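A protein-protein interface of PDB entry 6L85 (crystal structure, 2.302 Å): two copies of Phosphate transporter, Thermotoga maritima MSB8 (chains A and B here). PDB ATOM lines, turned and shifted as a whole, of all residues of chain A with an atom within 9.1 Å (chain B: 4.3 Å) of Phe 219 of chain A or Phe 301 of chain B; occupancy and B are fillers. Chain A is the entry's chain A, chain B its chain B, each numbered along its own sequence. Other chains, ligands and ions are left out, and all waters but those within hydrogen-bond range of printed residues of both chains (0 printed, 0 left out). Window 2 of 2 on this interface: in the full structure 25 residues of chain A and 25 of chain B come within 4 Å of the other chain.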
ATOM      1  N   SER A 171      24.463  23.320 -39.086  1.00  0.00           N
ATOM      2  CA  SER A 171      25.141  23.883 -37.935  1.00  0.00           C
ATOM      3  C   SER A 171      25.702  22.788 -37.027  1.00  0.00           C
ATOM      4  O   SER A 171      26.771  22.975 -36.415  1.00  0.00           O
ATOM      5  CB  SER A 171      24.178  24.768 -37.160  1.00  0.00           C
ATOM      6  OG  SER A 171      23.365  23.953 -36.344  1.00  0.00           O
ATOM      7  N   THR A 172      25.007  21.644 -36.946  1.00  0.00           N
ATOM      8  CA  THR A 172      25.561  20.525 -36.174  1.00  0.00           C
ATOM      9  C   THR A 172      26.849  19.960 -36.779  1.00  0.00           C
ATOM     10  O   THR A 172      27.513  19.153 -36.121  1.00  0.00           O
ATOM     11  CB  THR A 172      24.563  19.361 -36.017  1.00  0.00           C
ATOM     12  OG1 THR A 172      24.521  18.590 -37.223  1.00  0.00           O
ATOM     13  CG2 THR A 172      23.167  19.861 -35.671  1.00  0.00           C
ATOM     14  N   VAL A 173      27.204  20.329 -38.008  1.00  0.00           N
ATOM     15  CA  VAL A 173      28.472  19.934 -38.611  1.00  0.00           C
ATOM     16  C   VAL A 173      29.487  21.070 -38.568  1.00  0.00           C
ATOM     17  O   VAL A 173      30.673  20.845 -38.330  1.00  0.00           O
ATOM     18  CB  VAL A 173      28.263  19.460 -40.068  1.00  0.00           C
ATOM     19  CG1 VAL A 173      29.603  19.155 -40.725  1.00  0.00           C
ATOM     20  CG2 VAL A 173      27.338  18.258 -40.134  1.00  0.00           C
ATOM     21  N   PRO A 176      30.878  22.171 -34.596  1.00  0.00           N
ATOM     22  CA  PRO A 176      31.925  21.221 -34.165  1.00  0.00           C
ATOM     23  C   PRO A 176      33.199  21.336 -34.970  1.00  0.00           C
ATOM     24  O   PRO A 176      34.293  21.251 -34.406  1.00  0.00           O
ATOM     25  CB  PRO A 176      31.264  19.850 -34.357  1.00  0.00           C
ATOM     26  CG  PRO A 176      29.790  20.130 -34.217  1.00  0.00           C
ATOM     27  CD  PRO A 176      29.566  21.503 -34.754  1.00  0.00           C
ATOM     28  N   LEU A 211      39.313  14.994 -32.993  1.00  0.00           N
ATOM     29  CA  LEU A 211      38.276  13.984 -33.210  1.00  0.00           C
ATOM     30  C   LEU A 211      37.370  13.833 -31.997  1.00  0.00           C
ATOM     31  O   LEU A 211      36.130  13.799 -32.126  1.00  0.00           O
ATOM     32  CB  LEU A 211      38.918  12.645 -33.546  1.00  0.00           C
ATOM     33  CG  LEU A 211      39.607  12.666 -34.908  1.00  0.00           C
ATOM     34  CD1 LEU A 211      40.379  11.362 -35.162  1.00  0.00           C
ATOM     35  CD2 LEU A 211      38.546  12.920 -35.967  1.00  0.00           C
ATOM     36  N   VAL A 212      37.962  13.723 -30.804  1.00  0.00           N
ATOM     37  CA  VAL A 212      37.126  13.657 -29.601  1.00  0.00           C
ATOM     38  C   VAL A 212      36.262  14.913 -29.490  1.00  0.00           C
ATOM     39  O   VAL A 212      35.058  14.848 -29.192  1.00  0.00           O
ATOM     40  CB  VAL A 212      37.992  13.468 -28.345  1.00  0.00           C
ATOM     41  CG1 VAL A 212      37.092  13.406 -27.104  1.00  0.00           C
ATOM     42  CG2 VAL A 212      38.858  12.208 -28.473  1.00  0.00           C
ATOM     43  N   THR A 213      36.879  16.077 -29.702  1.00  0.00           N
ATOM     44  CA  THR A 213      36.151  17.335 -29.593  1.00  0.00           C
ATOM     45  C   THR A 213      34.989  17.382 -30.582  1.00  0.00           C
ATOM     46  O   THR A 213      33.861  17.691 -30.204  1.00  0.00           O
ATOM     47  CB  THR A 213      37.122  18.497 -29.796  1.00  0.00           C
ATOM     48  OG1 THR A 213      38.141  18.407 -28.795  1.00  0.00           O
ATOM     49  CG2 THR A 213      36.404  19.854 -29.670  1.00  0.00           C
ATOM     50  N   PHE A 214      35.241  17.031 -31.840  1.00  0.00           N
ATOM     51  CA  PHE A 214      34.184  17.030 -32.840  1.00  0.00           C
ATOM     52  C   PHE A 214      33.022  16.143 -32.415  1.00  0.00           C
ATOM     53  O   PHE A 214      31.856  16.552 -32.494  1.00  0.00           O
ATOM     54  CB  PHE A 214      34.733  16.580 -34.199  1.00  0.00           C
ATOM     55  CG  PHE A 214      33.761  16.812 -35.332  1.00  0.00           C
ATOM     56  CD1 PHE A 214      32.708  15.922 -35.554  1.00  0.00           C
ATOM     57  CD2 PHE A 214      33.867  17.940 -36.140  1.00  0.00           C
ATOM     58  CE1 PHE A 214      31.789  16.134 -36.567  1.00  0.00           C
ATOM     59  CE2 PHE A 214      32.943  18.169 -37.174  1.00  0.00           C
ATOM     60  CZ  PHE A 214      31.897  17.268 -37.382  1.00  0.00           C
ATOM     61  N   PHE A 215      33.314  14.915 -31.977  1.00  0.00           N
ATOM     62  CA  PHE A 215      32.239  14.013 -31.556  1.00  0.00           C
ATOM     63  C   PHE A 215      31.389  14.642 -30.456  1.00  0.00           C
ATOM     64  O   PHE A 215      30.152  14.726 -30.567  1.00  0.00           O
ATOM     65  CB  PHE A 215      32.840  12.681 -31.078  1.00  0.00           C
ATOM     66  CG  PHE A 215      31.822  11.571 -30.900  1.00  0.00           C
ATOM     67  CD1 PHE A 215      30.959  11.562 -29.813  1.00  0.00           C
ATOM     68  CD2 PHE A 215      31.719  10.548 -31.838  1.00  0.00           C
ATOM     69  CE1 PHE A 215      30.015  10.544 -29.653  1.00  0.00           C
ATOM     70  CE2 PHE A 215      30.777   9.525 -31.677  1.00  0.00           C
ATOM     71  CZ  PHE A 215      29.930   9.526 -30.587  1.00  0.00           C
ATOM     72  N   VAL A 216      32.041  15.088 -29.376  1.00  0.00           N
ATOM     73  CA  VAL A 216      31.288  15.591 -28.227  1.00  0.00           C
ATOM     74  C   VAL A 216      30.495  16.842 -28.606  1.00  0.00           C
ATOM     75  O   VAL A 216      29.320  16.997 -28.233  1.00  0.00           O
ATOM     76  CB  VAL A 216      32.231  15.862 -27.041  1.00  0.00           C
ATOM     77  CG1 VAL A 216      31.518  16.666 -25.973  1.00  0.00           C
ATOM     78  CG2 VAL A 216      32.783  14.539 -26.465  1.00  0.00           C
ATOM     79  N   VAL A 217      31.134  17.768 -29.330  1.00  0.00           N
ATOM     80  CA  VAL A 217      30.462  19.019 -29.659  1.00  0.00           C
ATOM     81  C   VAL A 217      29.305  18.745 -30.610  1.00  0.00           C
ATOM     82  O   VAL A 217      28.253  19.369 -30.511  1.00  0.00           O
ATOM     83  CB  VAL A 217      31.455  20.050 -30.246  1.00  0.00           C
ATOM     84  CG1 VAL A 217      30.695  21.336 -30.723  1.00  0.00           C
ATOM     85  CG2 VAL A 217      32.541  20.420 -29.233  1.00  0.00           C
ATOM     86  N   HIS A 218      29.472  17.791 -31.525  1.00  0.00           N
ATOM     87  CA  HIS A 218      28.396  17.453 -32.437  1.00  0.00           C
ATOM     88  C   HIS A 218      27.185  16.967 -31.672  1.00  0.00           C
ATOM     89  O   HIS A 218      26.066  17.437 -31.903  1.00  0.00           O
ATOM     90  CB  HIS A 218      28.874  16.405 -33.439  1.00  0.00           C
ATOM     91  CG  HIS A 218      27.768  15.793 -34.241  1.00  0.00           C
ATOM     92  ND1 HIS A 218      27.246  16.393 -35.371  1.00  0.00           N
ATOM     93  CD2 HIS A 218      27.086  14.631 -34.081  1.00  0.00           C
ATOM     94  CE1 HIS A 218      26.288  15.630 -35.868  1.00  0.00           C
ATOM     95  NE2 HIS A 218      26.175  14.553 -35.109  1.00  0.00           N
ATOM     96  N   PHE A 219      27.387  16.063 -30.712  1.00  0.00           N
ATOM     97  CA  PHE A 219      26.194  15.586 -30.017  1.00  0.00           C
ATOM     98  C   PHE A 219      25.594  16.644 -29.100  1.00  0.00           C
ATOM     99  O   PHE A 219      24.361  16.726 -28.990  1.00  0.00           O
ATOM    100  CB  PHE A 219      26.482  14.281 -29.286  1.00  0.00           C
ATOM    101  CG  PHE A 219      26.425  13.125 -30.199  1.00  0.00           C
ATOM    102  CD1 PHE A 219      25.201  12.588 -30.566  1.00  0.00           C
ATOM    103  CD2 PHE A 219      27.576  12.646 -30.789  1.00  0.00           C
ATOM    104  CE1 PHE A 219      25.131  11.555 -31.461  1.00  0.00           C
ATOM    105  CE2 PHE A 219      27.519  11.611 -31.688  1.00  0.00           C
ATOM    106  CZ  PHE A 219      26.292  11.059 -32.025  1.00  0.00           C
ATOM    107  N   ALA A 220      26.419  17.495 -28.478  1.00  0.00           N
ATOM    108  CA  ALA A 220      25.848  18.592 -27.693  1.00  0.00           C
ATOM    109  C   ALA A 220      25.042  19.547 -28.574  1.00  0.00           C
ATOM    110  O   ALA A 220      23.955  19.988 -28.186  1.00  0.00           O
ATOM    111  CB  ALA A 220      26.945  19.356 -26.948  1.00  0.00           C
ATOM    112  N   VAL A 221      25.567  19.894 -29.757  1.00  0.00           N
ATOM    113  CA  VAL A 221      24.851  20.798 -30.656  1.00  0.00           C
ATOM    114  C   VAL A 221      23.571  20.143 -31.157  1.00  0.00           C
ATOM    115  O   VAL A 221      22.559  20.815 -31.366  1.00  0.00           O
ATOM    116  CB  VAL A 221      25.737  21.235 -31.840  1.00  0.00           C
ATOM    117  CG1 VAL A 221      24.895  21.998 -32.866  1.00  0.00           C
ATOM    118  CG2 VAL A 221      26.902  22.095 -31.373  1.00  0.00           C
ATOM    119  N   ARG A 222      23.603  18.828 -31.376  1.00  0.00           N
ATOM    120  CA  ARG A 222      22.399  18.123 -31.798  1.00  0.00           C
ATOM    121  C   ARG A 222      21.314  18.225 -30.744  1.00  0.00           C
ATOM    122  O   ARG A 222      20.133  18.408 -31.071  1.00  0.00           O
ATOM    123  CB  ARG A 222      22.716  16.659 -32.092  1.00  0.00           C
ATOM    124  CG  ARG A 222      22.403  16.280 -33.497  1.00  0.00           C
ATOM    125  CD  ARG A 222      23.159  15.052 -33.888  1.00  0.00           C
ATOM    126  NE  ARG A 222      22.572  13.831 -33.347  1.00  0.00           N
ATOM    127  CZ  ARG A 222      22.826  12.622 -33.844  1.00  0.00           C
ATOM    128  NH1 ARG A 222      23.643  12.493 -34.891  1.00  0.00           N
ATOM    129  NH2 ARG A 222      22.267  11.542 -33.302  1.00  0.00           N
ATOM    130  N   LYS A 223      21.693  18.106 -29.470  1.00  0.00           N
ATOM    131  CA  LYS A 223      20.714  18.322 -28.405  1.00  0.00           C
ATOM    132  C   LYS A 223      20.208  19.765 -28.417  1.00  0.00           C
ATOM    133  O   LYS A 223      18.998  20.015 -28.352  1.00  0.00           O
ATOM    134  CB  LYS A 223      21.323  17.969 -27.048  1.00  0.00           C
ATOM    135  CG  LYS A 223      20.579  18.532 -25.828  1.00  0.00           C
ATOM    136  CD  LYS A 223      19.127  18.053 -25.737  1.00  0.00           C
ATOM    137  CE  LYS A 223      18.188  19.219 -25.390  1.00  0.00           C
ATOM    138  NZ  LYS A 223      16.741  18.943 -25.664  1.00  0.00           N
ATOM    139  N   LEU A 224      21.124  20.729 -28.529  1.00  0.00           N
ATOM    140  CA  LEU A 224      20.744  22.133 -28.374  1.00  0.00           C
ATOM    141  C   LEU A 224      19.884  22.647 -29.529  1.00  0.00           C
ATOM    142  O   LEU A 224      19.030  23.521 -29.327  1.00  0.00           O
ATOM    143  CB  LEU A 224      21.995  22.991 -28.244  1.00  0.00           C
ATOM    144  CG  LEU A 224      21.770  24.370 -27.634  1.00  0.00           C
ATOM    145  CD1 LEU A 224      20.874  24.304 -26.411  1.00  0.00           C
ATOM    146  CD2 LEU A 224      23.103  24.984 -27.287  1.00  0.00           C
ATOM    147  N   ILE A 225      20.097  22.130 -30.739  1.00  0.00           N
ATOM    148  CA  ILE A 225      19.448  22.684 -31.914  1.00  0.00           C
ATOM    149  C   ILE A 225      17.949  22.410 -31.924  1.00  0.00           C
ATOM    150  O   ILE A 225      17.211  23.068 -32.670  1.00  0.00           O
ATOM    151  CB  ILE A 225      20.147  22.138 -33.174  1.00  0.00           C
ATOM    152  CG1 ILE A 225      19.815  22.993 -34.402  1.00  0.00           C
ATOM    153  CG2 ILE A 225      19.788  20.678 -33.408  1.00  0.00           C
ATOM    154  CD1 ILE A 225      20.468  24.356 -34.425  1.00  0.00           C
ATOM    155  N   ASN A 226      17.473  21.469 -31.108  1.00  0.00           N
ATOM    156  CA  ASN A 226      16.055  21.144 -31.038  1.00  0.00           C
ATOM    157  C   ASN A 226      15.367  21.795 -29.845  1.00  0.00           C
ATOM    158  O   ASN A 226      14.232  21.434 -29.519  1.00  0.00           O
ATOM    159  CB  ASN A 226      15.863  19.627 -31.008  1.00  0.00           C
ATOM    160  CG  ASN A 226      16.188  18.977 -32.341  1.00  0.00           C
ATOM    161  OD1 ASN A 226      16.000  19.579 -33.404  1.00  0.00           O
ATOM    162  ND2 ASN A 226      16.675  17.743 -32.295  1.00  0.00           N
ATOM    163  N   VAL A 238      22.532  28.135 -30.691  1.00  0.00           N
ATOM    164  CA  VAL A 238      23.690  27.249 -30.674  1.00  0.00           C
ATOM    165  C   VAL A 238      24.987  28.054 -30.801  1.00  0.00           C
ATOM    166  O   VAL A 238      25.951  27.814 -30.060  1.00  0.00           O
ATOM    167  CB  VAL A 238      23.568  26.180 -31.777  1.00  0.00           C
ATOM    168  CG1 VAL A 238      24.876  25.497 -31.969  1.00  0.00           C
ATOM    169  CG2 VAL A 238      22.504  25.142 -31.401  1.00  0.00           C
ATOM    170  N   ARG B  39      23.189  11.392 -20.442  1.00  0.00           N
ATOM    171  CA  ARG B  39      23.790  11.844 -21.695  1.00  0.00           C
ATOM    172  C   ARG B  39      24.893  12.873 -21.451  1.00  0.00           C
ATOM    173  O   ARG B  39      25.976  12.805 -22.062  1.00  0.00           O
ATOM    174  CB  ARG B  39      22.695  12.423 -22.595  1.00  0.00           C
ATOM    175  CG  ARG B  39      23.187  13.348 -23.702  1.00  0.00           C
ATOM    176  CD  ARG B  39      24.129  12.635 -24.675  1.00  0.00           C
ATOM    177  NE  ARG B  39      23.433  11.825 -25.673  1.00  0.00           N
ATOM    178  CZ  ARG B  39      22.966  12.293 -26.827  1.00  0.00           C
ATOM    179  NH1 ARG B  39      23.119  13.579 -27.138  1.00  0.00           N
ATOM    180  NH2 ARG B  39      22.349  11.471 -27.670  1.00  0.00           N
ATOM    181  N   LEU B  43      29.031  12.584 -22.210  1.00  0.00           N
ATOM    182  CA  LEU B  43      29.861  13.507 -23.002  1.00  0.00           C
ATOM    183  C   LEU B  43      31.049  14.037 -22.194  1.00  0.00           C
ATOM    184  O   LEU B  43      32.206  14.096 -22.688  1.00  0.00           O
ATOM    185  CB  LEU B  43      28.998  14.660 -23.525  1.00  0.00           C
ATOM    186  CG  LEU B  43      27.902  14.238 -24.508  1.00  0.00           C
ATOM    187  CD1 LEU B  43      26.874  15.374 -24.791  1.00  0.00           C
ATOM    188  CD2 LEU B  43      28.501  13.703 -25.798  1.00  0.00           C
ATOM    189  N   MET B  46      33.580  11.308 -21.824  1.00  0.00           N
ATOM    190  CA  MET B  46      34.296  11.124 -23.080  1.00  0.00           C
ATOM    191  C   MET B  46      35.527  12.005 -23.133  1.00  0.00           C
ATOM    192  O   MET B  46      36.613  11.558 -23.522  1.00  0.00           O
ATOM    193  CB  MET B  46      33.387  11.446 -24.261  1.00  0.00           C
ATOM    194  CG  MET B  46      32.472  10.315 -24.637  1.00  0.00           C
ATOM    195  SD  MET B  46      31.572  10.744 -26.131  1.00  0.00           S
ATOM    196  CE  MET B  46      32.658  10.071 -27.384  1.00  0.00           C
ATOM    197  N   SER B 297      36.392   6.338 -24.760  1.00  0.00           N
ATOM    198  CA  SER B 297      35.382   7.384 -24.964  1.00  0.00           C
ATOM    199  C   SER B 297      34.176   6.857 -25.737  1.00  0.00           C
ATOM    200  O   SER B 297      33.016   7.110 -25.372  1.00  0.00           O
ATOM    201  CB  SER B 297      35.998   8.566 -25.715  1.00  0.00           C
ATOM    202  OG  SER B 297      36.845   9.292 -24.843  1.00  0.00           O
ATOM    203  N   LEU B 298      34.434   6.126 -26.815  1.00  0.00           N
ATOM    204  CA  LEU B 298      33.340   5.609 -27.622  1.00  0.00           C
ATOM    205  C   LEU B 298      32.541   4.555 -26.853  1.00  0.00           C
ATOM    206  O   LEU B 298      31.311   4.509 -26.954  1.00  0.00           O
ATOM    207  CB  LEU B 298      33.899   5.080 -28.949  1.00  0.00           C
ATOM    208  CG  LEU B 298      34.285   6.164 -29.980  1.00  0.00           C
ATOM    209  CD1 LEU B 298      34.978   5.588 -31.208  1.00  0.00           C
ATOM    210  CD2 LEU B 298      33.076   6.994 -30.447  1.00  0.00           C
ATOM    211  N   GLY B 299      33.208   3.727 -26.039  1.00  0.00           N
ATOM    212  CA  GLY B 299      32.476   2.783 -25.211  1.00  0.00           C
ATOM    213  C   GLY B 299      31.625   3.479 -24.167  1.00  0.00           C
ATOM    214  O   GLY B 299      30.514   3.039 -23.859  1.00  0.00           O
ATOM    215  N   VAL B 300      32.137   4.571 -23.596  1.00  0.00           N
ATOM    216  CA  VAL B 300      31.343   5.347 -22.652  1.00  0.00           C
ATOM    217  C   VAL B 300      30.073   5.830 -23.326  1.00  0.00           C
ATOM    218  O   VAL B 300      28.976   5.733 -22.763  1.00  0.00           O
ATOM    219  CB  VAL B 300      32.149   6.539 -22.105  1.00  0.00           C
ATOM    220  CG1 VAL B 300      31.172   7.630 -21.550  1.00  0.00           C
ATOM    221  CG2 VAL B 300      33.144   6.097 -21.057  1.00  0.00           C
ATOM    222  N   PHE B 301      30.201   6.343 -24.554  1.00  0.00           N
ATOM    223  CA  PHE B 301      29.039   6.935 -25.209  1.00  0.00           C
ATOM    224  C   PHE B 301      28.049   5.893 -25.721  1.00  0.00           C
ATOM    225  O   PHE B 301      26.840   6.075 -25.578  1.00  0.00           O
ATOM    226  CB  PHE B 301      29.466   7.833 -26.369  1.00  0.00           C
ATOM    227  CG  PHE B 301      28.319   8.570 -26.998  1.00  0.00           C
ATOM    228  CD1 PHE B 301      27.756   9.676 -26.370  1.00  0.00           C
ATOM    229  CD2 PHE B 301      27.776   8.139 -28.195  1.00  0.00           C
ATOM    230  CE1 PHE B 301      26.675  10.368 -26.953  1.00  0.00           C
ATOM    231  CE2 PHE B 301      26.697   8.821 -28.792  1.00  0.00           C
ATOM    232  CZ  PHE B 301      26.149   9.940 -28.171  1.00  0.00           C
ATOM    233  N   PHE B 302      28.520   4.829 -26.360  1.00  0.00           N
ATOM    234  CA  PHE B 302      27.601   3.912 -27.016  1.00  0.00           C
ATOM    235  C   PHE B 302      27.106   2.783 -26.133  1.00  0.00           C
ATOM    236  O   PHE B 302      26.087   2.161 -26.467  1.00  0.00           O
ATOM    237  CB  PHE B 302      28.240   3.297 -28.256  1.00  0.00           C
ATOM    238  CG  PHE B 302      28.303   4.235 -29.428  1.00  0.00           C
ATOM    239  CD1 PHE B 302      27.139   4.639 -30.078  1.00  0.00           C
ATOM    240  CD2 PHE B 302      29.524   4.715 -29.878  1.00  0.00           C
ATOM    241  CE1 PHE B 302      27.197   5.510 -31.161  1.00  0.00           C
ATOM    242  CE2 PHE B 302      29.595   5.577 -30.957  1.00  0.00           C
ATOM    243  CZ  PHE B 302      28.429   5.980 -31.603  1.00  0.00           C
ATOM    244  N   LEU B 303      27.797   2.462 -25.047  1.00  0.00           N
ATOM    245  CA  LEU B 303      27.327   1.311 -24.289  1.00  0.00           C
ATOM    246  C   LEU B 303      27.253   1.582 -22.791  1.00  0.00           C
ATOM    247  O   LEU B 303      26.413   0.999 -22.098  1.00  0.00           O
ATOM    248  CB  LEU B 303      28.212   0.098 -24.605  1.00  0.00           C
ATOM    249  CG  LEU B 303      27.806  -1.233 -23.971  1.00  0.00           C
ATOM    250  CD1 LEU B 303      26.309  -1.512 -24.194  1.00  0.00           C
ATOM    251  CD2 LEU B 303      28.672  -2.377 -24.513  1.00  0.00           C
ATOM    252  N   GLN B 305      26.090   3.958 -21.299  1.00  0.00           N
ATOM    253  CA  GLN B 305      24.859   4.696 -21.061  1.00  0.00           C
ATOM    254  C   GLN B 305      23.766   3.702 -20.690  1.00  0.00           C
ATOM    255  O   GLN B 305      22.576   3.986 -20.872  1.00  0.00           O
ATOM    256  CB  GLN B 305      24.471   5.518 -22.310  1.00  0.00           C
ATOM    257  CG  GLN B 305      25.195   6.876 -22.472  1.00  0.00           C
ATOM    258  CD  GLN B 305      24.443   7.884 -23.369  1.00  0.00           C
ATOM    259  OE1 GLN B 305      23.494   8.530 -22.933  1.00  0.00           O
ATOM    260  NE2 GLN B 305      24.891   8.036 -24.608  1.00  0.00           N
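No position is printed for both chains.
Along chain A the printed residues that touch a printed residue of chain B span positions 215 to 219. Printed residues of chain B that touch a printed residue of chain A: Arg 39, Leu 43, Met 46, Leu 298, Phe 301 and Phe 302. Along chain B the printed residues that touch a printed residue of chain A span positions 39 to 302. Among the printed residues, 8 pairs touch across the chains. Among the printed residues, no Asp or Glu carboxylate lies within 4 Å of a Lys or Arg side-chain nitrogen of the other chain.
Among the printed residues, pairs that only touch across the chains: Phe 215 of chain A with Met 46 of chain B, Phe 215 of chain A with Phe 301 of chain B, Phe 215 of chain A with Leu 298 of chain B, Phe 219 of chain A with Phe 301 of chain B, Val 216 of chain A with Met 46 of chain B, Val 216 of chain A with Leu 43 of chain B, Phe 219 of chain A with Arg 39 of chain B and Phe 215 of chain A with Phe 302 of chain B.
Phe 219 of chain A touches just these residues of chain B: Arg 39 (3.9 Å) and Phe 301 (3.7 Å). Printed residues of chain A within 4 Å of Arg 39 of chain B: Phe 219 (3.9 Å). Printed residues of chain A within 4 Å of Leu 298 of chain B: Phe 215 (3.6 Å). Val 300 of chain B touches none of the printed residues of chain A. The nearest residue of chain B that does not touch Phe 219 of chain A is Leu 43 of chain B (4.1 Å). The nearest printed residue of chain A that does not touch Met 46 of chain B is Val 212 of chain A (4.1 Å).
O of Met 46 of chain B sits at hydrogen-bond distance from OG of Ser 297 of chain B, 2.6 Å away. The backbone carbonyl oxygen (O) of Phe 301 of chain B lies within hydrogen-bond range of the side-chain amide nitrogen (NE2) of Gln 305 of chain B (2.9 Å).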
